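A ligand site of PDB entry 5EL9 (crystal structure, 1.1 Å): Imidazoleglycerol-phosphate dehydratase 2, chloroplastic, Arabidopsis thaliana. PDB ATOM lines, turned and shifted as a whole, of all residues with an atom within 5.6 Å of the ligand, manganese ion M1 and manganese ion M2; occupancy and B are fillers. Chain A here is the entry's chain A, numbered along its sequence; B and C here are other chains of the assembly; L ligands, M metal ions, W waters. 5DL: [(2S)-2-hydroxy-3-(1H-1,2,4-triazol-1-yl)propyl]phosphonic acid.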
ATOM      1  N   HIS A  45     -25.578   2.940  -2.449  1.00  0.00           N
ATOM      2  CA  HIS A  45     -26.151   3.952  -1.543  1.00  0.00           C
ATOM      3  C   HIS A  45     -27.282   4.735  -2.234  1.00  0.00           C
ATOM      4  O   HIS A  45     -28.276   5.082  -1.598  1.00  0.00           O
ATOM      5  CB  HIS A  45     -25.024   4.866  -1.049  1.00  0.00           C
ATOM      6  CG  HIS A  45     -25.456   5.964  -0.117  1.00  0.00           C
ATOM      7  ND1 HIS A  45     -26.290   5.812   0.952  1.00  0.00           N
ATOM      8  CD2 HIS A  45     -25.102   7.288  -0.107  1.00  0.00           C
ATOM      9  CE1 HIS A  45     -26.427   6.972   1.571  1.00  0.00           C
ATOM     10  NE2 HIS A  45     -25.729   7.893   0.935  1.00  0.00           N
ATOM     11  N   MET A  46     -27.103   5.001  -3.522  1.00  0.00           N
ATOM     12  CA  MET A  46     -28.160   5.693  -4.298  1.00  0.00           C
ATOM     13  C   MET A  46     -29.404   4.812  -4.478  1.00  0.00           C
ATOM     14  O   MET A  46     -30.527   5.267  -4.313  1.00  0.00           O
ATOM     15  CB  MET A  46     -27.634   6.151  -5.645  1.00  0.00           C
ATOM     16  CG  MET A  46     -26.553   7.215  -5.561  1.00  0.00           C
ATOM     17  SD  MET A  46     -26.996   8.694  -4.600  1.00  0.00           S
ATOM     18  CE  MET A  46     -26.290   8.278  -2.992  1.00  0.00           C
ATOM     19  N   GLN A  49     -31.683   4.832  -1.636  1.00  0.00           N
ATOM     20  CA  GLN A  49     -32.649   5.943  -1.581  1.00  0.00           C
ATOM     21  C   GLN A  49     -33.895   5.601  -2.384  1.00  0.00           C
ATOM     22  O   GLN A  49     -35.002   6.011  -2.042  1.00  0.00           O
ATOM     23  CB  GLN A  49     -32.034   7.251  -2.088  1.00  0.00           C
ATOM     24  CG  GLN A  49     -30.730   7.614  -1.389  1.00  0.00           C
ATOM     25  CD  GLN A  49     -30.799   7.500   0.098  1.00  0.00           C
ATOM     26  OE1 GLN A  49     -31.696   8.051   0.743  1.00  0.00           O
ATOM     27  NE2 GLN A  49     -29.856   6.796   0.681  1.00  0.00           N
ATOM     28  N   HIS A  53     -37.131   5.910  -0.097  1.00  0.00           N
ATOM     29  CA  HIS A  53     -38.027   7.046  -0.419  1.00  0.00           C
ATOM     30  C   HIS A  53     -39.106   6.743  -1.444  1.00  0.00           C
ATOM     31  O   HIS A  53     -40.185   7.326  -1.438  1.00  0.00           O
ATOM     32  CB  HIS A  53     -37.200   8.287  -0.739  1.00  0.00           C
ATOM     33  CG  HIS A  53     -36.428   8.719   0.456  1.00  0.00           C
ATOM     34  ND1 HIS A  53     -37.067   9.175   1.598  1.00  0.00           N
ATOM     35  CD2 HIS A  53     -35.123   8.569   0.777  1.00  0.00           C
ATOM     36  CE1 HIS A  53     -36.164   9.361   2.531  1.00  0.00           C
ATOM     37  NE2 HIS A  53     -34.983   8.989   2.064  1.00  0.00           N
ATOM     38  N   LEU A 105     -31.208  18.204  -0.803  1.00  0.00           N
ATOM     39  CA  LEU A 105     -30.324  17.622   0.196  1.00  0.00           C
ATOM     40  C   LEU A 105     -29.380  18.767   0.537  1.00  0.00           C
ATOM     41  O   LEU A 105     -28.510  19.132  -0.265  1.00  0.00           O
ATOM     42  CB  LEU A 105     -29.566  16.401  -0.309  1.00  0.00           C
ATOM     43  CG  LEU A 105     -28.963  15.539   0.786  1.00  0.00           C
ATOM     44  CD1 LEU A 105     -28.276  14.317   0.204  1.00  0.00           C
ATOM     45  CD2 LEU A 105     -28.065  16.256   1.770  1.00  0.00           C
ATOM     46  N   ASP A 106     -29.620  19.354   1.700  1.00  0.00           N
ATOM     47  CA  ASP A 106     -28.889  20.542   2.128  1.00  0.00           C
ATOM     48  C   ASP A 106     -28.971  21.600   1.022  1.00  0.00           C
ATOM     49  O   ASP A 106     -30.083  21.991   0.641  1.00  0.00           O
ATOM     50  CB  ASP A 106     -27.489  20.206   2.600  1.00  0.00           C
ATOM     51  CG  ASP A 106     -27.470  19.297   3.831  1.00  0.00           C
ATOM     52  OD1 ASP A 106     -28.559  18.924   4.348  1.00  0.00           O
ATOM     53  OD2 ASP A 106     -26.323  18.991   4.224  1.00  0.00           O
ATOM     54  N   HIS A 167     -21.952  14.758  -3.881  1.00  0.00           N
ATOM     55  CA  HIS A 167     -22.781  13.724  -3.217  1.00  0.00           C
ATOM     56  C   HIS A 167     -24.192  14.253  -2.953  1.00  0.00           C
ATOM     57  O   HIS A 167     -25.181  13.565  -3.211  1.00  0.00           O
ATOM     58  CB  HIS A 167     -22.067  13.282  -1.940  1.00  0.00           C
ATOM     59  CG  HIS A 167     -22.683  12.165  -1.120  1.00  0.00           C
ATOM     60  ND1 HIS A 167     -21.858  11.273  -0.504  1.00  0.00           N
ATOM     61  CD2 HIS A 167     -23.940  11.840  -0.715  1.00  0.00           C
ATOM     62  CE1 HIS A 167     -22.572  10.450   0.244  1.00  0.00           C
ATOM     63  NE2 HIS A 167     -23.846  10.778   0.147  1.00  0.00           N
ATOM     64  N   HIS A 168     -24.296  15.500  -2.502  1.00  0.00           N
ATOM     65  CA  HIS A 168     -25.623  16.087  -2.284  1.00  0.00           C
ATOM     66  C   HIS A 168     -26.433  16.193  -3.581  1.00  0.00           C
ATOM     67  O   HIS A 168     -27.621  15.871  -3.597  1.00  0.00           O
ATOM     68  CB  HIS A 168     -25.527  17.448  -1.645  1.00  0.00           C
ATOM     69  CG  HIS A 168     -25.000  17.429  -0.249  1.00  0.00           C
ATOM     70  ND1 HIS A 168     -24.789  18.581   0.460  1.00  0.00           N
ATOM     71  CD2 HIS A 168     -24.703  16.413   0.593  1.00  0.00           C
ATOM     72  CE1 HIS A 168     -24.379  18.259   1.684  1.00  0.00           C
ATOM     73  NE2 HIS A 168     -24.314  16.951   1.797  1.00  0.00           N
ATOM     74  N   GLU A 171     -27.395  12.520  -4.724  1.00  0.00           N
ATOM     75  CA  GLU A 171     -28.340  11.886  -3.819  1.00  0.00           C
ATOM     76  C   GLU A 171     -29.695  12.570  -3.829  1.00  0.00           C
ATOM     77  O   GLU A 171     -30.740  11.904  -3.828  1.00  0.00           O
ATOM     78  CB  GLU A 171     -27.769  11.780  -2.416  1.00  0.00           C
ATOM     79  CG  GLU A 171     -28.655  10.908  -1.536  1.00  0.00           C
ATOM     80  CD  GLU A 171     -28.151  10.745  -0.139  1.00  0.00           C
ATOM     81  OE1 GLU A 171     -26.916  10.633   0.042  1.00  0.00           O
ATOM     82  OE2 GLU A 171     -28.997  10.798   0.795  1.00  0.00           O
ATOM     83  N   LYS A 175     -33.330  10.823  -4.636  1.00  0.00           N
ATOM     84  CA  LYS A 175     -34.505  11.007  -3.790  1.00  0.00           C
ATOM     85  C   LYS A 175     -35.679  11.571  -4.549  1.00  0.00           C
ATOM     86  O   LYS A 175     -36.796  11.096  -4.404  1.00  0.00           O
ATOM     87  CB  LYS A 175     -34.135  11.914  -2.598  1.00  0.00           C
ATOM     88  CG  LYS A 175     -33.362  11.180  -1.545  1.00  0.00           C
ATOM     89  CD  LYS A 175     -32.656  12.139  -0.595  1.00  0.00           C
ATOM     90  CE  LYS A 175     -32.251  11.505   0.720  1.00  0.00           C
ATOM     91  NZ  LYS A 175     -31.232  12.310   1.422  1.00  0.00           N
ATOM     92  N   GLU B  19     -24.528   4.704   8.978  1.00  0.00           N
ATOM     93  CA  GLU B  19     -23.381   5.130   8.168  1.00  0.00           C
ATOM     94  C   GLU B  19     -22.056   5.239   8.923  1.00  0.00           C
ATOM     95  O   GLU B  19     -21.016   4.934   8.346  1.00  0.00           O
ATOM     96  CB  GLU B  19     -23.663   6.477   7.517  1.00  0.00           C
ATOM     97  CG  GLU B  19     -24.849   6.448   6.547  1.00  0.00           C
ATOM     98  CD  GLU B  19     -25.377   7.806   6.121  1.00  0.00           C
ATOM     99  OE1 GLU B  19     -25.051   8.818   6.765  1.00  0.00           O
ATOM    100  OE2 GLU B  19     -26.196   7.846   5.156  1.00  0.00           O
ATOM    101  N   HIS B  71     -17.422  11.311   2.818  1.00  0.00           N
ATOM    102  CA  HIS B  71     -18.438  12.303   3.192  1.00  0.00           C
ATOM    103  C   HIS B  71     -19.150  12.069   4.514  1.00  0.00           C
ATOM    104  O   HIS B  71     -19.186  12.979   5.358  1.00  0.00           O
ATOM    105  CB  HIS B  71     -19.442  12.383   2.041  1.00  0.00           C
ATOM    106  CG  HIS B  71     -20.439  13.491   2.176  1.00  0.00           C
ATOM    107  ND1 HIS B  71     -20.645  14.386   1.157  1.00  0.00           N
ATOM    108  CD2 HIS B  71     -21.329  13.831   3.132  1.00  0.00           C
ATOM    109  CE1 HIS B  71     -21.602  15.231   1.503  1.00  0.00           C
ATOM    110  NE2 HIS B  71     -22.025  14.922   2.702  1.00  0.00           N
ATOM    111  N   HIS B  72     -19.761  10.906   4.688  1.00  0.00           N
ATOM    112  CA  HIS B  72     -20.590  10.737   5.881  1.00  0.00           C
ATOM    113  C   HIS B  72     -19.705  10.822   7.149  1.00  0.00           C
ATOM    114  O   HIS B  72     -20.104  11.439   8.137  1.00  0.00           O
ATOM    115  CB  HIS B  72     -21.410   9.440   5.879  1.00  0.00           C
ATOM    116  CG  HIS B  72     -22.372   9.279   4.731  1.00  0.00           C
ATOM    117  ND1 HIS B  72     -22.706   8.033   4.266  1.00  0.00           N
ATOM    118  CD2 HIS B  72     -23.066  10.164   3.957  1.00  0.00           C
ATOM    119  CE1 HIS B  72     -23.573   8.162   3.277  1.00  0.00           C
ATOM    120  NE2 HIS B  72     -23.821   9.440   3.066  1.00  0.00           N
ATOM    121  N   GLU B  75     -18.689  14.511   7.817  1.00  0.00           N
ATOM    122  CA  GLU B  75     -19.848  15.257   8.327  1.00  0.00           C
ATOM    123  C   GLU B  75     -20.150  14.896   9.770  1.00  0.00           C
ATOM    124  O   GLU B  75     -20.387  15.760  10.609  1.00  0.00           O
ATOM    125  CB  GLU B  75     -21.037  14.976   7.431  1.00  0.00           C
ATOM    126  CG  GLU B  75     -22.351  15.572   7.936  1.00  0.00           C
ATOM    127  CD  GLU B  75     -23.448  15.568   6.896  1.00  0.00           C
ATOM    128  OE1 GLU B  75     -23.208  15.133   5.763  1.00  0.00           O
ATOM    129  OE2 GLU B  75     -24.552  16.076   7.250  1.00  0.00           O
ATOM    130  N   HIS B 143     -17.885  21.417   4.083  1.00  0.00           N
ATOM    131  CA  HIS B 143     -18.904  20.654   4.795  1.00  0.00           C
ATOM    132  C   HIS B 143     -18.522  20.435   6.261  1.00  0.00           C
ATOM    133  O   HIS B 143     -19.374  20.437   7.142  1.00  0.00           O
ATOM    134  CB  HIS B 143     -19.156  19.319   4.111  1.00  0.00           C
ATOM    135  CG  HIS B 143     -20.500  18.725   4.394  1.00  0.00           C
ATOM    136  ND1 HIS B 143     -21.155  18.835   5.590  1.00  0.00           N
ATOM    137  CD2 HIS B 143     -21.322  18.029   3.573  1.00  0.00           C
ATOM    138  CE1 HIS B 143     -22.320  18.212   5.491  1.00  0.00           C
ATOM    139  NE2 HIS B 143     -22.429  17.686   4.297  1.00  0.00           N
ATOM    140  N   ARG C  97     -41.796  13.434   5.271  1.00  0.00           N
ATOM    141  CA  ARG C  97     -40.443  14.031   5.425  1.00  0.00           C
ATOM    142  C   ARG C  97     -40.189  15.193   4.456  1.00  0.00           C
ATOM    143  O   ARG C  97     -39.667  16.223   4.868  1.00  0.00           O
ATOM    144  CB  ARG C  97     -39.333  12.975   5.331  1.00  0.00           C
ATOM    145  CG  ARG C  97     -37.952  13.569   5.393  1.00  0.00           C
ATOM    146  CD  ARG C  97     -36.838  12.534   5.295  1.00  0.00           C
ATOM    147  NE  ARG C  97     -35.572  13.200   5.035  1.00  0.00           N
ATOM    148  CZ  ARG C  97     -34.403  12.618   4.866  1.00  0.00           C
ATOM    149  NH1 ARG C  97     -34.244  11.316   5.032  1.00  0.00           N
ATOM    150  NH2 ARG C  97     -33.369  13.381   4.560  1.00  0.00           N
ATOM    151  N   ASP C 115     -37.136  19.589   3.401  1.00  0.00           N
ATOM    152  CA  ASP C 115     -36.803  18.267   3.890  1.00  0.00           C
ATOM    153  C   ASP C 115     -36.654  18.392   5.388  1.00  0.00           C
ATOM    154  O   ASP C 115     -35.777  19.112   5.860  1.00  0.00           O
ATOM    155  CB  ASP C 115     -35.509  17.765   3.215  1.00  0.00           C
ATOM    156  CG  ASP C 115     -34.977  16.481   3.788  1.00  0.00           C
ATOM    157  OD1 ASP C 115     -35.732  15.845   4.538  1.00  0.00           O
ATOM    158  OD2 ASP C 115     -33.818  16.104   3.459  1.00  0.00           O
ATOM    159  N   SER C 117     -35.052  17.069   7.682  1.00  0.00           N
ATOM    160  CA  SER C 117     -33.804  16.269   7.725  1.00  0.00           C
ATOM    161  C   SER C 117     -33.097  16.221   9.057  1.00  0.00           C
ATOM    162  O   SER C 117     -32.312  15.316   9.304  1.00  0.00           O
ATOM    163  CB  SER C 117     -32.772  16.920   6.738  1.00  0.00           C
ATOM    164  OG  SER C 117     -32.556  18.270   7.060  1.00  0.00           O
ATOM    165  N   ARG C 119     -31.109  18.744   9.486  1.00  0.00           N
ATOM    166  CA  ARG C 119     -29.947  19.561   9.080  1.00  0.00           C
ATOM    167  C   ARG C 119     -30.452  20.925   8.630  1.00  0.00           C
ATOM    168  O   ARG C 119     -31.154  21.031   7.641  1.00  0.00           O
ATOM    169  CB  ARG C 119     -29.231  18.897   7.917  1.00  0.00           C
ATOM    170  CG  ARG C 119     -28.626  17.545   8.245  1.00  0.00           C
ATOM    171  CD  ARG C 119     -27.882  16.976   7.049  1.00  0.00           C
ATOM    172  NE  ARG C 119     -28.776  16.564   5.961  1.00  0.00           N
ATOM    173  CZ  ARG C 119     -29.227  15.343   5.748  1.00  0.00           C
ATOM    174  NH1 ARG C 119     -28.846  14.307   6.505  1.00  0.00           N
ATOM    175  NH2 ARG C 119     -30.062  15.114   4.738  1.00  0.00           N
ATOM    176  N   PRO C 196     -38.135   7.679   8.011  1.00  0.00           N
ATOM    177  CA  PRO C 196     -37.902   7.831   6.580  1.00  0.00           C
ATOM    178  C   PRO C 196     -36.467   8.296   6.287  1.00  0.00           C
ATOM    179  O   PRO C 196     -36.241   9.399   5.813  1.00  0.00           O
ATOM    180  CB  PRO C 196     -38.942   8.882   6.167  1.00  0.00           C
ATOM    181  CG  PRO C 196     -39.087   9.722   7.412  1.00  0.00           C
ATOM    182  CD  PRO C 196     -38.971   8.749   8.555  1.00  0.00           C
ATOM    183  N   SER C 197     -35.520   7.422   6.554  1.00  0.00           N
ATOM    184  CA  SER C 197     -34.116   7.670   6.304  1.00  0.00           C
ATOM    185  C   SER C 197     -33.365   6.381   6.172  1.00  0.00           C
ATOM    186  O   SER C 197     -33.469   5.517   7.033  1.00  0.00           O
ATOM    187  CB  SER C 197     -33.459   8.449   7.451  1.00  0.00           C
ATOM    188  OG  SER C 197     -32.065   8.593   7.252  1.00  0.00           O
ATOM    189  N   SER C 198     -32.530   6.287   5.140  1.00  0.00           N
ATOM    190  CA  SER C 198     -31.656   5.123   4.983  1.00  0.00           C
ATOM    191  C   SER C 198     -30.637   4.953   6.108  1.00  0.00           C
ATOM    192  O   SER C 198     -30.127   3.864   6.299  1.00  0.00           O
ATOM    193  CB  SER C 198     -30.938   5.186   3.640  1.00  0.00           C
ATOM    194  OG  SER C 198     -30.080   6.306   3.544  1.00  0.00           O
ATOM    195  N   LYS C 199     -30.332   6.034   6.856  1.00  0.00           N
ATOM    196  CA  LYS C 199     -29.315   5.941   7.905  1.00  0.00           C
ATOM    197  C   LYS C 199     -29.920   5.578   9.255  1.00  0.00           C
ATOM    198  O   LYS C 199     -29.181   5.395  10.231  1.00  0.00           O
ATOM    199  CB  LYS C 199     -28.454   7.183   8.004  1.00  0.00           C
ATOM    200  CG  LYS C 199     -29.070   8.382   8.708  1.00  0.00           C
ATOM    201  CD  LYS C 199     -28.210   9.640   8.610  1.00  0.00           C
ATOM    202  CE  LYS C 199     -28.758  10.826   9.367  1.00  0.00           C
ATOM    203  NZ  LYS C 199     -30.094  11.257   8.913  1.00  0.00           N
ATOM    204  N   VAL C 201     -32.121   7.177  11.346  1.00  0.00           N
ATOM    205  CA  VAL C 201     -32.401   8.212  12.344  1.00  0.00           C
ATOM    206  C   VAL C 201     -32.451   9.547  11.611  1.00  0.00           C
ATOM    207  O   VAL C 201     -31.771   9.702  10.607  1.00  0.00           O
ATOM    208  CB  VAL C 201     -31.327   8.203  13.460  1.00  0.00           C
ATOM    209  CG1 VAL C 201     -29.945   8.568  12.905  1.00  0.00           C
ATOM    210  CG2 VAL C 201     -31.704   9.094  14.636  1.00  0.00           C
ATOM    211  N   LEU C 202     -33.211  10.485  12.149  1.00  0.00           N
ATOM    212  CA  LEU C 202     -33.220  11.879  11.695  1.00  0.00           C
ATOM    213  C   LEU C 202     -32.976  12.708  12.960  1.00  0.00           C
ATOM    214  O   LEU C 202     -33.638  12.507  13.977  1.00  0.00           O
ATOM    215  CB  LEU C 202     -34.560  12.259  11.050  1.00  0.00           C
ATOM    216  CG  LEU C 202     -34.788  11.607   9.693  1.00  0.00           C
ATOM    217  CD1 LEU C 202     -36.227  11.836   9.237  1.00  0.00           C
ATOM    218  CD2 LEU C 202     -33.819  12.116   8.640  1.00  0.00           C
HETATM  219  N1  5DL L   1     -25.558  12.126   2.389  1.00  0.00           N
HETATM  220  C3  5DL L   1     -26.103  13.778   3.772  1.00  0.00           C
HETATM  221  N2  5DL L   1     -26.507  12.622   3.228  1.00  0.00           N
HETATM  222  C8  5DL L   1     -29.192  10.088   4.167  1.00  0.00           C
HETATM  223  C7  5DL L   1     -27.777  10.660   4.120  1.00  0.00           C
HETATM  224  C6  5DL L   1     -27.790  11.986   3.442  1.00  0.00           C
HETATM  225  C5  5DL L   1     -24.577  13.041   2.482  1.00  0.00           C
HETATM  226  O10 5DL L   1     -30.790  12.277   4.098  1.00  0.00           O
HETATM  227  P9  5DL L   1     -30.440  11.130   5.019  1.00  0.00           P
HETATM  228  O11 5DL L   1     -29.832  11.661   6.294  1.00  0.00           O
HETATM  229  O12 5DL L   1     -31.643  10.232   5.216  1.00  0.00           O
HETATM  230  O13 5DL L   1     -26.889   9.768   3.420  1.00  0.00           O
HETATM  231  N4  5DL L   1     -24.882  14.056   3.316  1.00  0.00           N
HETATM  232 MN    MN M   1     -23.742  15.946   3.727  1.00  0.00          MN
HETATM  233 MN    MN M   2     -25.501  10.027   1.550  1.00  0.00          MN
HETATM  234  O   HOH W   1     -25.558  16.559   4.792  1.00  0.00           O
HETATM  235  O   HOH W   2     -32.502   8.527   3.323  1.00  0.00           O
HETATM  236  O   HOH W   3     -25.822  11.503   6.843  1.00  0.00           O
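O11 of the ligand is in salt-bridge range of NH1 of Arg 119 of chain C, at 2.8 Å. An oxygen (O13) of the ligand lies close to the side-chain carboxylate (OE2) of Glu 19 of chain B, at 2.7 Å. O12 of the ligand lies within hydrogen-bond range of OG of Ser 197 of chain C, 2.6 Å away. An oxygen (O11) of the ligand is in salt-bridge range of the side-chain amino group of Lys 199 of chain C. The side-chain amino group (NZ) of Lys 175 lies within salt-bridge range of an oxygen (O10) of the ligand (2.7 Å). The guanidinium group (NH1) of Arg 97 of chain C is in salt-bridge range of an oxygen (O12) of the ligand (2.8 Å).
Water W1 lies within hydrogen-bond range of the side-chain carboxylate of Asp 106, the side-chain carboxylate of Glu 75 of chain B and the guanidinium group of Arg 119 of chain C. Water W2 lies within hydrogen-bond range of an oxygen (O12) of the ligand (2.7 Å), the side-chain amide oxygen of Gln 49 (2.7 Å), a ring nitrogen (NE2) of His 53 (2.8 Å) and the backbone NH of Ser 198 of chain C (2.9 Å).
Residues that only touch the ligand: Leu 105 and Ser 198 of chain C. Hydrophobic or aromatic side chains that line the ligand: His 45, Leu 105, His 167, His 168, His 71 of chain B and His 72 of chain B. Within 4 Å of the ligand: His 45, Leu 105, His 167, His 168, Glu 171, Lys 175, Glu 19 of chain B, His 71 of chain B, His 72 of chain B, Glu 75 of chain B, Arg 97 of chain C, Arg 119 of chain C, Ser 197 of chain C, Ser 198 of chain C and Lys 199 of chain C. The nearest printed residue that does not touch the ligand is Leu 202 of chain C (4.5 Å).
Manganese ion M1 is bound by water W1 (2.2 Å), N4 of the ligand (2.2 Å), NE2 of His 71 of chain B (2.2 Å), NE2 of His 168 (2.2 Å), NE2 of His 143 of chain B (2.3 Å) and OE1 of Glu 75 of chain B (2.3 Å).
Manganese ion M2 is bound by OE1 of Glu 171 (2.2 Å), NE2 of His 45 (2.2 Å), N1 of the ligand (2.3 Å), NE2 of His 167 (2.3 Å), NE2 of His 72 of chain B (2.3 Å) and O13 of the ligand (2.3 Å). Manganese ion M2 has six donor atoms within binding distance.
Of the 25 residues printed, 4 come within 4 Å of manganese ion M1. The nearest printed residue that does not touch manganese ion M1 is Asp 106 (4.02 Å).
Of the 25 residues printed, 4 come within 4 Å of manganese ion M2.
NE of Arg 97 of chain C is in salt-bridge range of OD1 of Asp 115 of chain C, 2.7 Å away. O of His 45 sits at hydrogen-bond distance from NE2 of Gln 49. The side-chain hydroxyl of Ser 197 of chain C is in hydrogen-bond range of the backbone NH of Lys 199 of chain C (3.1 Å). The side-chain amino group of Lys 175 lies within salt-bridge range of the side-chain carboxylate of Glu 171 (2.8 Å). The backbone NH (N) of Arg 119 of chain C is in hydrogen-bond range of the side-chain hydroxyl (OG) of Ser 117 of chain C (2.9 Å). The side-chain carboxylate (OD1) of Asp 106 lies within salt-bridge range of the guanidinium group (NE) of Arg 119 of chain C. The side-chain hydroxyl of Ser 198 of chain C lies within hydrogen-bond range of the side-chain amide nitrogen of Gln 49 (2.9 Å). NH1 of Arg 97 of chain C is in hydrogen-bond range of O of Pro 196 of chain C, 2.9 Å away.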
